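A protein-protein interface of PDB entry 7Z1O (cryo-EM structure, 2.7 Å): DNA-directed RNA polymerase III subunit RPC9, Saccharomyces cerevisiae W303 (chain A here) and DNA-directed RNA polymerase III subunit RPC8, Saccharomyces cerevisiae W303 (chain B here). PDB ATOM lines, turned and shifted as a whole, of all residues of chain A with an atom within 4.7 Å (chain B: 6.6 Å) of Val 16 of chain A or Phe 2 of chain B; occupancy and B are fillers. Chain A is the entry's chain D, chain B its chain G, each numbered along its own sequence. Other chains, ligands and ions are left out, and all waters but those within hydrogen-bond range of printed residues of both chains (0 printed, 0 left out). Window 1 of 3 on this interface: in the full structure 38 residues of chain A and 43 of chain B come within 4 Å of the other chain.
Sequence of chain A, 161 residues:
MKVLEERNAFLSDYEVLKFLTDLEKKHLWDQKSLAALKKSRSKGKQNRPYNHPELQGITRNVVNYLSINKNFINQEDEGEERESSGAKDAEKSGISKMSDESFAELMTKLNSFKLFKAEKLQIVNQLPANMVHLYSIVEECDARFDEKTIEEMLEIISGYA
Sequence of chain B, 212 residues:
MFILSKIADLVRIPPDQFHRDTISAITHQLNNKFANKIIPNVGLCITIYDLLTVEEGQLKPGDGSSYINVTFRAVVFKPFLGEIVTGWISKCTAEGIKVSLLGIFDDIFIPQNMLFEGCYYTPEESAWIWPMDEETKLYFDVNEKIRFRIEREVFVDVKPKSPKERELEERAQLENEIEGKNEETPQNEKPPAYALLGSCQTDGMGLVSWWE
N of Leu 11 of chain A lies within hydrogen-bond range of O of Phe 2 of chain B (3.2 Å). SD of Met 1 of chain B lies close to OD1 of Asp 13 of chain A, 3.6 Å away.
The backbone carbonyl oxygen of Met 1 of chain B is in hydrogen-bond range of the backbone NH of Lys 78 of chain B, 2.8 Å away. The backbone NH (N) of Met 1 of chain B lies within hydrogen-bond range of the side-chain carboxylate (OE2) of Glu 83 of chain B. N of Val 76 of chain B is in hydrogen-bond range of O of Ile 3 of chain B, 2.9 Å away. The backbone NH (N) of Ile 46 of chain B is in hydrogen-bond range of the backbone carbonyl oxygen (O) of Val 75 of chain B (2.8 Å).
Phe 10 of chain A touches Ile 3 of chain B. Leu 11 of chain A touches Leu 4 of chain B. Leu 11 of chain A touches Val 75 of chain B (CD1 to CG2, 3.7 Å). Asp 13 of chain A touches Phe 2 of chain B. Phe 2 of chain B touches Val 16 of chain A. CG2 of Val 62 of chain A touches CD1 of Ile 46 of chain B (3.9 Å). Val 62 of chain A touches Ile 104 of chain B.
Printed residues of chain B within 4 Å of Phe 10 of chain A: Ile 3 (3.7 Å). Printed residues of chain B within 4 Å of Leu 11 of chain A: Phe 2 (3.1 Å), Leu 4 (3.7 Å) and Val 75 (3.7 Å). Phe 2 of chain B touches three residues of chain A. Printed residues of chain A within 4 Å of Ile 3 of chain B: Phe 10. Of the printed residues of chain A, Leu 4 of chain B touches Leu 11. Leu 44 of chain B touches none of the printed residues of chain A. Of the printed residues of chain A, Ile 104 of chain B touches Val 62 (3.7 Å). The nearest residue of chain A that does not touch Phe 2 of chain B is Leu 66 of chain A (4.1 Å).
Of the 13 printed residues of chain A, 5 touch a printed residue of chain B. Along chain A the printed residues that touch a printed residue of chain B span positions 10 to 62. Of the 13 printed residues of chain B, 7 touch a printed residue of chain A. Printed residues of chain B that touch a printed residue of chain A: Met 1, Phe 2, Ile 3, Leu 4, Ile 46, Val 75 and Ile 104. Among the printed residues, 9 pairs touch across the chains.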
ATOM      1  N   PHE A  10     -33.067  -3.783 -33.044  1.00  0.00           N
ATOM      2  CA  PHE A  10     -32.459  -2.463 -33.132  1.00  0.00           C
ATOM      3  C   PHE A  10     -32.943  -1.610 -31.968  1.00  0.00           C
ATOM      4  O   PHE A  10     -34.144  -1.567 -31.682  1.00  0.00           O
ATOM      5  CB  PHE A  10     -32.803  -1.785 -34.458  1.00  0.00           C
ATOM      6  CG  PHE A  10     -31.753  -1.954 -35.517  1.00  0.00           C
ATOM      7  CD1 PHE A  10     -30.481  -1.441 -35.335  1.00  0.00           C
ATOM      8  CD2 PHE A  10     -32.043  -2.611 -36.700  1.00  0.00           C
ATOM      9  CE1 PHE A  10     -29.513  -1.590 -36.309  1.00  0.00           C
ATOM     10  CE2 PHE A  10     -31.080  -2.761 -37.679  1.00  0.00           C
ATOM     11  CZ  PHE A  10     -29.814  -2.251 -37.482  1.00  0.00           C
ATOM     12  N   LEU A  11     -32.011  -0.937 -31.303  1.00  0.00           N
ATOM     13  CA  LEU A  11     -32.320  -0.078 -30.168  1.00  0.00           C
ATOM     14  C   LEU A  11     -32.074   1.372 -30.557  1.00  0.00           C
ATOM     15  O   LEU A  11     -30.982   1.717 -31.019  1.00  0.00           O
ATOM     16  CB  LEU A  11     -31.476  -0.447 -28.948  1.00  0.00           C
ATOM     17  CG  LEU A  11     -31.842  -1.713 -28.176  1.00  0.00           C
ATOM     18  CD1 LEU A  11     -31.055  -1.766 -26.882  1.00  0.00           C
ATOM     19  CD2 LEU A  11     -33.332  -1.766 -27.900  1.00  0.00           C
ATOM     20  N   SER A  12     -33.088   2.210 -30.374  1.00  0.00           N
ATOM     21  CA  SER A  12     -32.905   3.640 -30.539  1.00  0.00           C
ATOM     22  C   SER A  12     -32.156   4.212 -29.340  1.00  0.00           C
ATOM     23  O   SER A  12     -32.001   3.562 -28.301  1.00  0.00           O
ATOM     24  CB  SER A  12     -34.254   4.339 -30.702  1.00  0.00           C
ATOM     25  OG  SER A  12     -34.946   4.403 -29.468  1.00  0.00           O
ATOM     26  N   ASP A  13     -31.674   5.446 -29.497  1.00  0.00           N
ATOM     27  CA  ASP A  13     -30.974   6.105 -28.399  1.00  0.00           C
ATOM     28  C   ASP A  13     -31.911   6.402 -27.237  1.00  0.00           C
ATOM     29  O   ASP A  13     -31.474   6.427 -26.080  1.00  0.00           O
ATOM     30  CB  ASP A  13     -30.313   7.392 -28.892  1.00  0.00           C
ATOM     31  CG  ASP A  13     -28.949   7.147 -29.507  1.00  0.00           C
ATOM     32  OD1 ASP A  13     -28.555   5.968 -29.631  1.00  0.00           O
ATOM     33  OD2 ASP A  13     -28.274   8.132 -29.872  1.00  0.00           O
ATOM     34  N   TYR A  14     -33.197   6.627 -27.523  1.00  0.00           N
ATOM     35  CA  TYR A  14     -34.162   6.883 -26.459  1.00  0.00           C
ATOM     36  C   TYR A  14     -34.337   5.666 -25.559  1.00  0.00           C
ATOM     37  O   TYR A  14     -34.400   5.800 -24.332  1.00  0.00           O
ATOM     38  CB  TYR A  14     -35.506   7.299 -27.061  1.00  0.00           C
ATOM     39  CG  TYR A  14     -36.666   7.188 -26.099  1.00  0.00           C
ATOM     40  CD1 TYR A  14     -36.772   8.038 -25.007  1.00  0.00           C
ATOM     41  CD2 TYR A  14     -37.653   6.231 -26.283  1.00  0.00           C
ATOM     42  CE1 TYR A  14     -37.831   7.938 -24.127  1.00  0.00           C
ATOM     43  CE2 TYR A  14     -38.715   6.123 -25.407  1.00  0.00           C
ATOM     44  CZ  TYR A  14     -38.799   6.979 -24.332  1.00  0.00           C
ATOM     45  OH  TYR A  14     -39.855   6.874 -23.457  1.00  0.00           O
ATOM     46  N   GLU A  15     -34.418   4.471 -26.152  1.00  0.00           N
ATOM     47  CA  GLU A  15     -34.598   3.255 -25.365  1.00  0.00           C
ATOM     48  C   GLU A  15     -33.395   2.999 -24.467  1.00  0.00           C
ATOM     49  O   GLU A  15     -33.545   2.674 -23.283  1.00  0.00           O
ATOM     50  CB  GLU A  15     -34.832   2.063 -26.290  1.00  0.00           C
ATOM     51  CG  GLU A  15     -36.226   1.981 -26.877  1.00  0.00           C
ATOM     52  CD  GLU A  15     -36.506   0.633 -27.507  1.00  0.00           C
ATOM     53  OE1 GLU A  15     -36.169  -0.396 -26.885  1.00  0.00           O
ATOM     54  OE2 GLU A  15     -37.049   0.600 -28.630  1.00  0.00           O
ATOM     55  N   VAL A  16     -32.189   3.146 -25.021  1.00  0.00           N
ATOM     56  CA  VAL A  16     -30.969   2.936 -24.246  1.00  0.00           C
ATOM     57  C   VAL A  16     -30.859   3.974 -23.137  1.00  0.00           C
ATOM     58  O   VAL A  16     -30.502   3.649 -21.996  1.00  0.00           O
ATOM     59  CB  VAL A  16     -29.741   2.957 -25.176  1.00  0.00           C
ATOM     60  CG1 VAL A  16     -28.452   3.060 -24.379  1.00  0.00           C
ATOM     61  CG2 VAL A  16     -29.727   1.721 -26.057  1.00  0.00           C
ATOM     62  N   LEU A  17     -31.181   5.233 -23.448  1.00  0.00           N
ATOM     63  CA  LEU A  17     -31.125   6.294 -22.447  1.00  0.00           C
ATOM     64  C   LEU A  17     -32.103   6.033 -21.308  1.00  0.00           C
ATOM     65  O   LEU A  17     -31.749   6.165 -20.130  1.00  0.00           O
ATOM     66  CB  LEU A  17     -31.411   7.642 -23.108  1.00  0.00           C
ATOM     67  CG  LEU A  17     -31.413   8.885 -22.219  1.00  0.00           C
ATOM     68  CD1 LEU A  17     -30.144   8.955 -21.393  1.00  0.00           C
ATOM     69  CD2 LEU A  17     -31.578  10.141 -23.058  1.00  0.00           C
ATOM     70  N   LYS A  18     -33.337   5.642 -21.642  1.00  0.00           N
ATOM     71  CA  LYS A  18     -34.333   5.363 -20.611  1.00  0.00           C
ATOM     72  C   LYS A  18     -33.932   4.162 -19.763  1.00  0.00           C
ATOM     73  O   LYS A  18     -34.049   4.198 -18.530  1.00  0.00           O
ATOM     74  CB  LYS A  18     -35.700   5.132 -21.252  1.00  0.00           C
ATOM     75  CG  LYS A  18     -36.823   4.945 -20.247  1.00  0.00           C
ATOM     76  CD  LYS A  18     -38.120   4.550 -20.931  1.00  0.00           C
ATOM     77  CE  LYS A  18     -39.221   4.300 -19.913  1.00  0.00           C
ATOM     78  NZ  LYS A  18     -40.423   3.679 -20.535  1.00  0.00           N
ATOM     79  N   PHE A  19     -33.442   3.097 -20.403  1.00  0.00           N
ATOM     80  CA  PHE A  19     -33.036   1.904 -19.670  1.00  0.00           C
ATOM     81  C   PHE A  19     -31.868   2.195 -18.736  1.00  0.00           C
ATOM     82  O   PHE A  19     -31.852   1.733 -17.591  1.00  0.00           O
ATOM     83  CB  PHE A  19     -32.676   0.786 -20.648  1.00  0.00           C
ATOM     84  CG  PHE A  19     -31.947  -0.361 -20.016  1.00  0.00           C
ATOM     85  CD1 PHE A  19     -32.584  -1.183 -19.102  1.00  0.00           C
ATOM     86  CD2 PHE A  19     -30.625  -0.620 -20.336  1.00  0.00           C
ATOM     87  CE1 PHE A  19     -31.915  -2.240 -18.518  1.00  0.00           C
ATOM     88  CE2 PHE A  19     -29.951  -1.675 -19.756  1.00  0.00           C
ATOM     89  CZ  PHE A  19     -30.597  -2.486 -18.846  1.00  0.00           C
ATOM     90  N   LEU A  20     -30.893   2.982 -19.195  1.00  0.00           N
ATOM     91  CA  LEU A  20     -29.737   3.258 -18.352  1.00  0.00           C
ATOM     92  C   LEU A  20     -30.063   4.250 -17.243  1.00  0.00           C
ATOM     93  O   LEU A  20     -29.500   4.149 -16.149  1.00  0.00           O
ATOM     94  CB  LEU A  20     -28.570   3.751 -19.202  1.00  0.00           C
ATOM     95  CG  LEU A  20     -27.971   2.635 -20.058  1.00  0.00           C
ATOM     96  CD1 LEU A  20     -26.897   3.173 -20.969  1.00  0.00           C
ATOM     97  CD2 LEU A  20     -27.425   1.515 -19.184  1.00  0.00           C
ATOM     98  N   VAL A  62     -22.150   6.783 -21.237  1.00  0.00           N
ATOM     99  CA  VAL A  62     -23.211   6.689 -22.236  1.00  0.00           C
ATOM    100  C   VAL A  62     -24.318   7.700 -21.950  1.00  0.00           C
ATOM    101  O   VAL A  62     -24.846   8.333 -22.874  1.00  0.00           O
ATOM    102  CB  VAL A  62     -23.756   5.250 -22.322  1.00  0.00           C
ATOM    103  CG1 VAL A  62     -24.950   5.191 -23.256  1.00  0.00           C
ATOM    104  CG2 VAL A  62     -22.681   4.307 -22.822  1.00  0.00           C
ATOM    105  N   LEU A  66     -25.385  10.627 -24.579  1.00  0.00           N
ATOM    106  CA  LEU A  66     -26.729  10.738 -25.133  1.00  0.00           C
ATOM    107  C   LEU A  66     -27.512  11.899 -24.536  1.00  0.00           C
ATOM    108  O   LEU A  66     -28.550  12.277 -25.089  1.00  0.00           O
ATOM    109  CB  LEU A  66     -27.496   9.432 -24.926  1.00  0.00           C
ATOM    110  CG  LEU A  66     -26.886   8.174 -25.544  1.00  0.00           C
ATOM    111  CD1 LEU A  66     -27.799   6.977 -25.336  1.00  0.00           C
ATOM    112  CD2 LEU A  66     -26.606   8.384 -27.021  1.00  0.00           C
ATOM    113  N   MET B   1     -26.703   2.261 -34.028  1.00  0.00           N
ATOM    114  CA  MET B   1     -25.655   2.566 -33.063  1.00  0.00           C
ATOM    115  C   MET B   1     -25.594   1.491 -31.985  1.00  0.00           C
ATOM    116  O   MET B   1     -24.560   0.853 -31.785  1.00  0.00           O
ATOM    117  CB  MET B   1     -25.892   3.937 -32.430  1.00  0.00           C
ATOM    118  CG  MET B   1     -24.783   4.392 -31.500  1.00  0.00           C
ATOM    119  SD  MET B   1     -25.111   6.017 -30.791  1.00  0.00           S
ATOM    120  CE  MET B   1     -24.861   7.066 -32.220  1.00  0.00           C
ATOM    121  N   PHE B   2     -26.712   1.295 -31.293  1.00  0.00           N
ATOM    122  CA  PHE B   2     -26.838   0.289 -30.250  1.00  0.00           C
ATOM    123  C   PHE B   2     -27.778  -0.810 -30.723  1.00  0.00           C
ATOM    124  O   PHE B   2     -28.875  -0.527 -31.214  1.00  0.00           O
ATOM    125  CB  PHE B   2     -27.370   0.901 -28.951  1.00  0.00           C
ATOM    126  CG  PHE B   2     -26.460   1.928 -28.348  1.00  0.00           C
ATOM    127  CD1 PHE B   2     -25.227   1.567 -27.835  1.00  0.00           C
ATOM    128  CD2 PHE B   2     -26.842   3.257 -28.288  1.00  0.00           C
ATOM    129  CE1 PHE B   2     -24.391   2.513 -27.276  1.00  0.00           C
ATOM    130  CE2 PHE B   2     -26.009   4.207 -27.730  1.00  0.00           C
ATOM    131  CZ  PHE B   2     -24.782   3.832 -27.224  1.00  0.00           C
ATOM    132  N   ILE B   3     -27.349  -2.063 -30.577  1.00  0.00           N
ATOM    133  CA  ILE B   3     -28.149  -3.218 -30.965  1.00  0.00           C
ATOM    134  C   ILE B   3     -28.197  -4.195 -29.798  1.00  0.00           C
ATOM    135  O   ILE B   3     -27.516  -4.027 -28.785  1.00  0.00           O
ATOM    136  CB  ILE B   3     -27.607  -3.916 -32.231  1.00  0.00           C
ATOM    137  CG1 ILE B   3     -26.202  -4.443 -31.972  1.00  0.00           C
ATOM    138  CG2 ILE B   3     -27.626  -2.972 -33.425  1.00  0.00           C
ATOM    139  CD1 ILE B   3     -25.668  -5.336 -33.052  1.00  0.00           C
ATOM    140  N   LEU B   4     -29.029  -5.221 -29.948  1.00  0.00           N
ATOM    141  CA  LEU B   4     -29.207  -6.260 -28.941  1.00  0.00           C
ATOM    142  C   LEU B   4     -28.610  -7.559 -29.459  1.00  0.00           C
ATOM    143  O   LEU B   4     -28.927  -7.990 -30.573  1.00  0.00           O
ATOM    144  CB  LEU B   4     -30.685  -6.451 -28.603  1.00  0.00           C
ATOM    145  CG  LEU B   4     -31.304  -5.444 -27.637  1.00  0.00           C
ATOM    146  CD1 LEU B   4     -32.754  -5.792 -27.372  1.00  0.00           C
ATOM    147  CD2 LEU B   4     -30.515  -5.416 -26.345  1.00  0.00           C
ATOM    148  N   LEU B  44     -18.729  -3.700 -28.775  1.00  0.00           N
ATOM    149  CA  LEU B  44     -18.474  -3.310 -27.394  1.00  0.00           C
ATOM    150  C   LEU B  44     -19.773  -3.417 -26.612  1.00  0.00           C
ATOM    151  O   LEU B  44     -20.761  -2.760 -26.955  1.00  0.00           O
ATOM    152  CB  LEU B  44     -17.906  -1.889 -27.323  1.00  0.00           C
ATOM    153  CG  LEU B  44     -17.395  -1.358 -25.980  1.00  0.00           C
ATOM    154  CD1 LEU B  44     -16.198  -0.459 -26.208  1.00  0.00           C
ATOM    155  CD2 LEU B  44     -18.466  -0.588 -25.232  1.00  0.00           C
ATOM    156  N   ILE B  46     -22.323  -2.869 -23.510  1.00  0.00           N
ATOM    157  CA  ILE B  46     -22.589  -1.800 -22.554  1.00  0.00           C
ATOM    158  C   ILE B  46     -23.147  -2.389 -21.267  1.00  0.00           C
ATOM    159  O   ILE B  46     -22.522  -2.293 -20.204  1.00  0.00           O
ATOM    160  CB  ILE B  46     -23.560  -0.758 -23.140  1.00  0.00           C
ATOM    161  CG1 ILE B  46     -22.967  -0.112 -24.391  1.00  0.00           C
ATOM    162  CG2 ILE B  46     -23.894   0.300 -22.104  1.00  0.00           C
ATOM    163  CD1 ILE B  46     -21.737   0.713 -24.121  1.00  0.00           C
ATOM    164  N   VAL B  75     -27.004  -5.139 -24.559  1.00  0.00           N
ATOM    165  CA  VAL B  75     -26.896  -3.958 -25.407  1.00  0.00           C
ATOM    166  C   VAL B  75     -25.438  -3.793 -25.811  1.00  0.00           C
ATOM    167  O   VAL B  75     -24.576  -3.532 -24.965  1.00  0.00           O
ATOM    168  CB  VAL B  75     -27.407  -2.707 -24.681  1.00  0.00           C
ATOM    169  CG1 VAL B  75     -27.367  -1.502 -25.605  1.00  0.00           C
ATOM    170  CG2 VAL B  75     -28.807  -2.936 -24.142  1.00  0.00           C
ATOM    171  N   VAL B  76     -25.155  -3.939 -27.102  1.00  0.00           N
ATOM    172  CA  VAL B  76     -23.797  -3.825 -27.615  1.00  0.00           C
ATOM    173  C   VAL B  76     -23.742  -2.700 -28.641  1.00  0.00           C
ATOM    174  O   VAL B  76     -24.695  -2.477 -29.400  1.00  0.00           O
ATOM    175  CB  VAL B  76     -23.277  -5.157 -28.200  1.00  0.00           C
ATOM    176  CG1 VAL B  76     -23.227  -6.221 -27.118  1.00  0.00           C
ATOM    177  CG2 VAL B  76     -24.142  -5.631 -29.333  1.00  0.00           C
ATOM    178  N   PHE B  77     -22.627  -1.977 -28.635  1.00  0.00           N
ATOM    179  CA  PHE B  77     -22.454  -0.761 -29.422  1.00  0.00           C
ATOM    180  C   PHE B  77     -21.849  -1.151 -30.767  1.00  0.00           C
ATOM    181  O   PHE B  77     -20.646  -1.397 -30.874  1.00  0.00           O
ATOM    182  CB  PHE B  77     -21.588   0.226 -28.645  1.00  0.00           C
ATOM    183  CG  PHE B  77     -21.056   1.368 -29.458  1.00  0.00           C
ATOM    184  CD1 PHE B  77     -21.871   2.436 -29.790  1.00  0.00           C
ATOM    185  CD2 PHE B  77     -19.726   1.400 -29.847  1.00  0.00           C
ATOM    186  CE1 PHE B  77     -21.380   3.498 -30.518  1.00  0.00           C
ATOM    187  CE2 PHE B  77     -19.231   2.459 -30.578  1.00  0.00           C
ATOM    188  CZ  PHE B  77     -20.057   3.510 -30.910  1.00  0.00           C
ATOM    189  N   LYS B  78     -22.696  -1.234 -31.793  1.00  0.00           N
ATOM    190  CA  LYS B  78     -22.292  -1.629 -33.144  1.00  0.00           C
ATOM    191  C   LYS B  78     -22.830  -0.622 -34.148  1.00  0.00           C
ATOM    192  O   LYS B  78     -23.954  -0.768 -34.647  1.00  0.00           O
ATOM    193  CB  LYS B  78     -22.788  -3.032 -33.494  1.00  0.00           C
ATOM    194  CG  LYS B  78     -21.964  -3.721 -34.572  1.00  0.00           C
ATOM    195  CD  LYS B  78     -22.408  -5.157 -34.798  1.00  0.00           C
ATOM    196  CE  LYS B  78     -21.706  -5.764 -36.004  1.00  0.00           C
ATOM    197  NZ  LYS B  78     -22.662  -6.350 -36.982  1.00  0.00           N
ATOM    198  N   PRO B  79     -22.063   0.420 -34.463  1.00  0.00           N
ATOM    199  CA  PRO B  79     -22.470   1.329 -35.544  1.00  0.00           C
ATOM    200  C   PRO B  79     -22.409   0.622 -36.888  1.00  0.00           C
ATOM    201  O   PRO B  79     -21.349   0.173 -37.326  1.00  0.00           O
ATOM    202  CB  PRO B  79     -21.447   2.467 -35.454  1.00  0.00           C
ATOM    203  CG  PRO B  79     -20.885   2.370 -34.088  1.00  0.00           C
ATOM    204  CD  PRO B  79     -20.878   0.917 -33.749  1.00  0.00           C
ATOM    205  N   GLU B  83     -23.903   4.639 -41.124  1.00  0.00           N
ATOM    206  CA  GLU B  83     -24.427   5.456 -40.041  1.00  0.00           C
ATOM    207  C   GLU B  83     -23.452   6.573 -39.700  1.00  0.00           C
ATOM    208  O   GLU B  83     -22.248   6.343 -39.556  1.00  0.00           O
ATOM    209  CB  GLU B  83     -24.693   4.604 -38.800  1.00  0.00           C
ATOM    210  CG  GLU B  83     -25.528   5.304 -37.740  1.00  0.00           C
ATOM    211  CD  GLU B  83     -25.624   4.511 -36.452  1.00  0.00           C
ATOM    212  OE1 GLU B  83     -24.843   3.552 -36.284  1.00  0.00           O
ATOM    213  OE2 GLU B  83     -26.481   4.847 -35.607  1.00  0.00           O
ATOM    214  N   ILE B 104     -16.704   6.914 -24.334  1.00  0.00           N
ATOM    215  CA  ILE B 104     -17.289   5.608 -24.635  1.00  0.00           C
ATOM    216  C   ILE B 104     -16.312   4.758 -25.433  1.00  0.00           C
ATOM    217  O   ILE B 104     -16.048   3.597 -25.099  1.00  0.00           O
ATOM    218  CB  ILE B 104     -18.618   5.780 -25.393  1.00  0.00           C
ATOM    219  CG1 ILE B 104     -19.688   6.387 -24.492  1.00  0.00           C
ATOM    220  CG2 ILE B 104     -19.091   4.447 -25.958  1.00  0.00           C
ATOM    221  CD1 ILE B 104     -21.009   6.567 -25.196  1.00  0.00           C
